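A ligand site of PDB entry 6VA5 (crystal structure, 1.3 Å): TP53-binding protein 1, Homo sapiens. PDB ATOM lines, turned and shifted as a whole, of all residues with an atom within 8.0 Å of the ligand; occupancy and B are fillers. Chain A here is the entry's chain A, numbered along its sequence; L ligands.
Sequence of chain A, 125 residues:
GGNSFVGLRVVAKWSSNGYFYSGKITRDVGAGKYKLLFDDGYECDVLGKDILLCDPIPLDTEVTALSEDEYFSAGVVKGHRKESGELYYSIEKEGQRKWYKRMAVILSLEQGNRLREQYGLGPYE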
ATOM      1  N   ALA A  12      -1.693  25.479  21.347  1.00  0.00           N
ATOM      2  CA  ALA A  12      -0.548  24.718  20.814  1.00  0.00           C
ATOM      3  C   ALA A  12       0.053  23.809  21.878  1.00  0.00           C
ATOM      4  O   ALA A  12       0.098  24.169  23.065  1.00  0.00           O
ATOM      5  CB  ALA A  12       0.530  25.667  20.333  1.00  0.00           C
ATOM      6  N   LYS A  13       0.556  22.662  21.449  1.00  0.00           N
ATOM      7  CA  LYS A  13       1.211  21.754  22.380  1.00  0.00           C
ATOM      8  C   LYS A  13       2.402  22.464  23.005  1.00  0.00           C
ATOM      9  O   LYS A  13       3.270  23.026  22.325  1.00  0.00           O
ATOM     10  CB  LYS A  13       1.700  20.500  21.667  1.00  0.00           C
ATOM     11  CG  LYS A  13       2.088  19.428  22.666  1.00  0.00           C
ATOM     12  CD  LYS A  13       2.571  18.167  21.999  1.00  0.00           C
ATOM     13  CE  LYS A  13       4.000  18.293  21.560  1.00  0.00           C
ATOM     14  NZ  LYS A  13       4.530  16.982  21.130  1.00  0.00           N
ATOM     15  N   TRP A  14       2.480  22.423  24.337  1.00  0.00           N
ATOM     16  CA  TRP A  14       3.620  22.996  25.058  1.00  0.00           C
ATOM     17  C   TRP A  14       4.751  21.988  25.077  1.00  0.00           C
ATOM     18  O   TRP A  14       4.592  20.865  25.546  1.00  0.00           O
ATOM     19  CB  TRP A  14       3.232  23.392  26.494  1.00  0.00           C
ATOM     20  CG  TRP A  14       4.447  23.685  27.330  1.00  0.00           C
ATOM     21  CD1 TRP A  14       4.966  22.893  28.303  1.00  0.00           C
ATOM     22  CD2 TRP A  14       5.359  24.771  27.175  1.00  0.00           C
ATOM     23  NE1 TRP A  14       6.130  23.428  28.781  1.00  0.00           N
ATOM     24  CE2 TRP A  14       6.400  24.583  28.102  1.00  0.00           C
ATOM     25  CE3 TRP A  14       5.373  25.919  26.377  1.00  0.00           C
ATOM     26  CZ2 TRP A  14       7.472  25.487  28.235  1.00  0.00           C
ATOM     27  CZ3 TRP A  14       6.441  26.817  26.497  1.00  0.00           C
ATOM     28  CH2 TRP A  14       7.468  26.583  27.432  1.00  0.00           C
ATOM     29  N   SER A  15       5.922  22.406  24.582  1.00  0.00           N
ATOM     30  CA  SER A  15       7.175  21.620  24.632  1.00  0.00           C
ATOM     31  C   SER A  15       6.901  20.164  24.238  1.00  0.00           C
ATOM     32  O   SER A  15       6.342  19.934  23.164  1.00  0.00           O
ATOM     33  CB  SER A  15       7.810  21.817  26.009  1.00  0.00           C
ATOM     34  OG  SER A  15       9.142  21.344  26.008  1.00  0.00           O
ATOM     35  N   SER A  16       7.254  19.209  25.095  1.00  0.00           N
ATOM     36  CA  SER A  16       6.899  17.804  24.867  1.00  0.00           C
ATOM     37  C   SER A  16       5.979  17.270  25.968  1.00  0.00           C
ATOM     38  O   SER A  16       6.085  16.113  26.398  1.00  0.00           O
ATOM     39  CB  SER A  16       8.163  16.958  24.726  1.00  0.00           C
ATOM     40  OG  SER A  16       8.953  17.391  23.614  1.00  0.00           O
ATOM     41  N   ASN A  17       5.070  18.128  26.413  1.00  0.00           N
ATOM     42  CA  ASN A  17       4.071  17.816  27.433  1.00  0.00           C
ATOM     43  C   ASN A  17       2.838  17.089  26.873  1.00  0.00           C
ATOM     44  O   ASN A  17       2.726  16.816  25.667  1.00  0.00           O
ATOM     45  CB  ASN A  17       3.583  19.131  28.104  1.00  0.00           C
ATOM     46  CG  ASN A  17       4.398  19.576  29.296  1.00  0.00           C
ATOM     47  OD1 ASN A  17       3.842  20.114  30.235  1.00  0.00           O
ATOM     48  ND2 ASN A  17       5.723  19.460  29.225  1.00  0.00           N
ATOM     49  N   GLY A  18       1.874  16.826  27.752  1.00  0.00           N
ATOM     50  CA  GLY A  18       0.644  16.166  27.392  1.00  0.00           C
ATOM     51  C   GLY A  18      -0.534  17.076  27.049  1.00  0.00           C
ATOM     52  O   GLY A  18      -1.618  16.568  26.807  1.00  0.00           O
ATOM     53  N   TYR A  19      -0.318  18.386  27.101  1.00  0.00           N
ATOM     54  CA  TYR A  19      -1.406  19.353  26.900  1.00  0.00           C
ATOM     55  C   TYR A  19      -0.996  20.459  25.943  1.00  0.00           C
ATOM     56  O   TYR A  19       0.185  20.849  25.846  1.00  0.00           O
ATOM     57  CB  TYR A  19      -1.915  19.964  28.221  1.00  0.00           C
ATOM     58  CG  TYR A  19      -2.862  19.025  28.924  1.00  0.00           C
ATOM     59  CD1 TYR A  19      -2.387  17.951  29.696  1.00  0.00           C
ATOM     60  CD2 TYR A  19      -4.242  19.154  28.791  1.00  0.00           C
ATOM     61  CE1 TYR A  19      -3.270  17.059  30.283  1.00  0.00           C
ATOM     62  CE2 TYR A  19      -5.115  18.272  29.379  1.00  0.00           C
ATOM     63  CZ  TYR A  19      -4.613  17.233  30.145  1.00  0.00           C
ATOM     64  OH  TYR A  19      -5.469  16.313  30.744  1.00  0.00           O
ATOM     65  N   PHE A  20      -2.008  20.970  25.252  1.00  0.00           N
ATOM     66  CA  PHE A  20      -1.980  22.201  24.462  1.00  0.00           C
ATOM     67  C   PHE A  20      -2.488  23.359  25.323  1.00  0.00           C
ATOM     68  O   PHE A  20      -3.508  23.217  26.023  1.00  0.00           O
ATOM     69  CB  PHE A  20      -2.918  22.142  23.241  1.00  0.00           C
ATOM     70  CG  PHE A  20      -2.564  21.165  22.147  1.00  0.00           C
ATOM     71  CD1 PHE A  20      -2.306  19.815  22.358  1.00  0.00           C
ATOM     72  CD2 PHE A  20      -2.660  21.605  20.824  1.00  0.00           C
ATOM     73  CE1 PHE A  20      -2.053  18.980  21.293  1.00  0.00           C
ATOM     74  CE2 PHE A  20      -2.416  20.751  19.754  1.00  0.00           C
ATOM     75  CZ  PHE A  20      -2.103  19.454  19.992  1.00  0.00           C
ATOM     76  N   TYR A  21      -1.805  24.505  25.195  1.00  0.00           N
ATOM     77  CA  TYR A  21      -2.119  25.722  25.955  1.00  0.00           C
ATOM     78  C   TYR A  21      -2.218  26.906  25.006  1.00  0.00           C
ATOM     79  O   TYR A  21      -1.671  26.874  23.903  1.00  0.00           O
ATOM     80  CB  TYR A  21      -1.014  26.005  26.974  1.00  0.00           C
ATOM     81  CG  TYR A  21      -0.800  24.947  28.030  1.00  0.00           C
ATOM     82  CD1 TYR A  21      -0.069  23.782  27.753  1.00  0.00           C
ATOM     83  CD2 TYR A  21      -1.305  25.098  29.308  1.00  0.00           C
ATOM     84  CE1 TYR A  21       0.138  22.828  28.719  1.00  0.00           C
ATOM     85  CE2 TYR A  21      -1.104  24.139  30.285  1.00  0.00           C
ATOM     86  CZ  TYR A  21      -0.386  22.999  29.978  1.00  0.00           C
ATOM     87  OH  TYR A  21      -0.185  22.031  30.951  1.00  0.00           O
ATOM     88  N   SER A  22      -2.917  27.954  25.450  1.00  0.00           N
ATOM     89  CA  SER A  22      -3.124  29.139  24.631  1.00  0.00           C
ATOM     90  C   SER A  22      -1.857  30.001  24.493  1.00  0.00           C
ATOM     91  O   SER A  22      -1.083  30.135  25.449  1.00  0.00           O
ATOM     92  CB  SER A  22      -4.245  29.956  25.261  1.00  0.00           C
ATOM     93  OG  SER A  22      -4.467  31.162  24.572  1.00  0.00           O
ATOM     94  N   GLY A  23      -1.673  30.591  23.310  1.00  0.00           N
ATOM     95  CA  GLY A  23      -0.521  31.463  23.079  1.00  0.00           C
ATOM     96  C   GLY A  23      -0.667  32.242  21.808  1.00  0.00           C
ATOM     97  O   GLY A  23      -1.729  32.336  21.226  1.00  0.00           O
ATOM     98  N   LEU A  37       4.798  32.651  22.145  1.00  0.00           N
ATOM     99  CA  LEU A  37       4.684  33.219  23.468  1.00  0.00           C
ATOM    100  C   LEU A  37       3.356  32.720  24.005  1.00  0.00           C
ATOM    101  O   LEU A  37       2.277  33.105  23.534  1.00  0.00           O
ATOM    102  CB  LEU A  37       4.706  34.746  23.408  1.00  0.00           C
ATOM    103  CG  LEU A  37       4.450  35.468  24.734  1.00  0.00           C
ATOM    104  CD1 LEU A  37       5.455  35.093  25.821  1.00  0.00           C
ATOM    105  CD2 LEU A  37       4.431  36.985  24.500  1.00  0.00           C
ATOM    106  N   PHE A  38       3.433  31.866  25.026  1.00  0.00           N
ATOM    107  CA  PHE A  38       2.228  31.358  25.654  1.00  0.00           C
ATOM    108  C   PHE A  38       1.652  32.420  26.565  1.00  0.00           C
ATOM    109  O   PHE A  38       2.379  33.296  27.038  1.00  0.00           O
ATOM    110  CB  PHE A  38       2.520  30.035  26.359  1.00  0.00           C
ATOM    111  CG  PHE A  38       2.705  28.912  25.386  1.00  0.00           C
ATOM    112  CD1 PHE A  38       3.911  28.738  24.700  1.00  0.00           C
ATOM    113  CD2 PHE A  38       1.631  28.056  25.092  1.00  0.00           C
ATOM    114  CE1 PHE A  38       4.055  27.738  23.773  1.00  0.00           C
ATOM    115  CE2 PHE A  38       1.788  27.045  24.167  1.00  0.00           C
ATOM    116  CZ  PHE A  38       3.006  26.873  23.523  1.00  0.00           C
ATOM    117  N   ASP A  39       0.343  32.336  26.796  1.00  0.00           N
ATOM    118  CA  ASP A  39      -0.333  33.359  27.576  1.00  0.00           C
ATOM    119  C   ASP A  39       0.147  33.422  29.019  1.00  0.00           C
ATOM    120  O   ASP A  39       0.031  34.473  29.648  1.00  0.00           O
ATOM    121  CB  ASP A  39      -1.850  33.153  27.495  1.00  0.00           C
ATOM    122  CG  ASP A  39      -2.398  33.376  26.099  1.00  0.00           C
ATOM    123  OD1 ASP A  39      -1.760  34.009  25.244  1.00  0.00           O
ATOM    124  OD2 ASP A  39      -3.515  32.941  25.843  1.00  0.00           O
ATOM    125  N   ASP A  40       0.697  32.321  29.546  1.00  0.00           N
ATOM    126  CA  ASP A  40       1.261  32.342  30.906  1.00  0.00           C
ATOM    127  C   ASP A  40       2.647  32.950  30.970  1.00  0.00           C
ATOM    128  O   ASP A  40       3.154  33.099  32.085  1.00  0.00           O
ATOM    129  CB  ASP A  40       1.210  30.968  31.572  1.00  0.00           C
ATOM    130  CG  ASP A  40       2.123  29.929  30.941  1.00  0.00           C
ATOM    131  OD1 ASP A  40       2.827  30.216  29.946  1.00  0.00           O
ATOM    132  OD2 ASP A  40       2.132  28.802  31.511  1.00  0.00           O
ATOM    133  N   GLY A  41       3.249  33.311  29.836  1.00  0.00           N
ATOM    134  CA  GLY A  41       4.536  33.989  29.771  1.00  0.00           C
ATOM    135  C   GLY A  41       5.679  33.129  29.265  1.00  0.00           C
ATOM    136  O   GLY A  41       6.736  33.653  28.914  1.00  0.00           O
ATOM    137  N   TYR A  42       5.498  31.810  29.254  1.00  0.00           N
ATOM    138  CA  TYR A  42       6.545  30.913  28.765  1.00  0.00           C
ATOM    139  C   TYR A  42       6.618  30.955  27.243  1.00  0.00           C
ATOM    140  O   TYR A  42       5.632  31.272  26.571  1.00  0.00           O
ATOM    141  CB  TYR A  42       6.257  29.492  29.230  1.00  0.00           C
ATOM    142  CG  TYR A  42       6.607  29.189  30.672  1.00  0.00           C
ATOM    143  CD1 TYR A  42       5.841  29.671  31.729  1.00  0.00           C
ATOM    144  CD2 TYR A  42       7.663  28.340  30.982  1.00  0.00           C
ATOM    145  CE1 TYR A  42       6.159  29.373  33.036  1.00  0.00           C
ATOM    146  CE2 TYR A  42       7.997  28.039  32.270  1.00  0.00           C
ATOM    147  CZ  TYR A  42       7.228  28.537  33.289  1.00  0.00           C
ATOM    148  OH  TYR A  42       7.560  28.196  34.595  1.00  0.00           O
ATOM    149  N   GLU A  43       7.807  30.632  26.726  1.00  0.00           N
ATOM    150  CA  GLU A  43       8.050  30.602  25.284  1.00  0.00           C
ATOM    151  C   GLU A  43       8.681  29.287  24.908  1.00  0.00           C
ATOM    152  O   GLU A  43       9.487  28.742  25.669  1.00  0.00           O
ATOM    153  CB  GLU A  43       9.006  31.729  24.878  1.00  0.00           C
ATOM    154  CG  GLU A  43       8.437  33.109  25.100  1.00  0.00           C
ATOM    155  CD  GLU A  43       9.374  34.222  24.730  1.00  0.00           C
ATOM    156  OE1 GLU A  43      10.550  34.183  25.123  1.00  0.00           O
ATOM    157  OE2 GLU A  43       8.917  35.152  24.037  1.00  0.00           O
ATOM    158  N   CYS A  44       8.316  28.761  23.749  1.00  0.00           N
ATOM    159  CA  CYS A  44       9.072  27.654  23.133  1.00  0.00           C
ATOM    160  C   CYS A  44       8.814  27.606  21.665  1.00  0.00           C
ATOM    161  O   CYS A  44       7.924  28.314  21.165  1.00  0.00           O
ATOM    162  CB  CYS A  44       8.753  26.313  23.793  1.00  0.00           C
ATOM    163  SG  CYS A  44       7.181  25.569  23.322  1.00  0.00           S
ATOM    164  N   MET A 103      -6.568  31.472  29.056  1.00  0.00           N
ATOM    165  CA  MET A 103      -5.368  30.672  29.371  1.00  0.00           C
ATOM    166  C   MET A 103      -5.635  29.472  30.281  1.00  0.00           C
ATOM    167  O   MET A 103      -4.805  28.576  30.386  1.00  0.00           O
ATOM    168  CB  MET A 103      -4.270  31.567  29.927  1.00  0.00           C
ATOM    169  CG  MET A 103      -4.558  32.028  31.333  1.00  0.00           C
ATOM    170  SD  MET A 103      -3.370  33.180  31.993  1.00  0.00           S
ATOM    171  CE  MET A 103      -2.017  32.090  32.161  1.00  0.00           C
ATOM    172  N   ILE A 106      -7.462  24.327  28.311  1.00  0.00           N
ATOM    173  CA  ILE A 106      -6.364  23.589  27.702  1.00  0.00           C
ATOM    174  C   ILE A 106      -6.924  22.346  27.032  1.00  0.00           C
ATOM    175  O   ILE A 106      -8.103  22.005  27.219  1.00  0.00           O
ATOM    176  CB  ILE A 106      -5.334  23.202  28.763  1.00  0.00           C
ATOM    177  CG1 ILE A 106      -5.972  22.331  29.846  1.00  0.00           C
ATOM    178  CG2 ILE A 106      -4.666  24.450  29.339  1.00  0.00           C
ATOM    179  CD1 ILE A 106      -4.993  21.955  30.885  1.00  0.00           C
HETATM  180  C1  LIG L   1       4.955  25.140  34.150  1.00  0.00           C
HETATM  181  C2  LIG L   1       4.743  24.419  32.978  1.00  0.00           C
HETATM  182  C3  LIG L   1       4.819  26.213  31.306  1.00  0.00           C
HETATM  183  N1  LIG L   1       4.155  25.011  31.816  1.00  0.00           N
HETATM  184  C4  LIG L   1       4.259  26.553  29.943  1.00  0.00           C
HETATM  185  C5  LIG L   1       2.265  27.100  28.672  1.00  0.00           C
HETATM  186  N2  LIG L   1       2.817  26.790  30.017  1.00  0.00           N
HETATM  187  C6  LIG L   1       2.157  25.608  30.581  1.00  0.00           C
HETATM  188  C7  LIG L   1       2.724  25.282  31.937  1.00  0.00           C
HETATM  189  N3  LIG L   1       4.804  22.337  31.789  1.00  0.00           N
HETATM  190  C8  LIG L   1       5.041  23.049  32.903  1.00  0.00           C
HETATM  191  C9  LIG L   1       5.453  24.491  35.274  1.00  0.00           C
HETATM  192  C10 LIG L   1       5.764  23.146  35.216  1.00  0.00           C
HETATM  193  C11 LIG L   1       5.565  22.432  34.054  1.00  0.00           C
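The side-chain amide oxygen (OD1) of Asn 17 is in hydrogen-bond range of a nitrogen (N3) of the ligand, at 2.9 Å. OD2 of Asp 40 is in salt-bridge range of N2 of the ligand, 2.6 Å away.
NE1 of Trp 14 sits close to N3 of the ligand, at 3.5 Å. Residues that only touch the ligand: Tyr 42 (3.5 Å), Tyr 21 (3.6 Å) and Phe 38 (3.7 Å). Hydrophobic or aromatic side chains within 4 Å of the ligand: Trp 14, Tyr 21, Phe 38 and Tyr 42. Within 4 Å of the ligand: Trp 14, Asn 17, Tyr 21, Phe 38, Asp 40 and Tyr 42. The nearest printed residue that does not touch the ligand is Ser 22 (5.6 Å).
The backbone carbonyl oxygen of Tyr 19 lies within hydrogen-bond range of the backbone NH of Trp 14, 3.2 Å away. The side-chain carboxylate (OD1) of Asp 40 lies within hydrogen-bond range of the backbone NH (N) of Tyr 42 (3.2 Å). The backbone NH (N) of Tyr 21 lies within hydrogen-bond range of the backbone carbonyl oxygen (O) of Ala 12 (2.9 Å).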
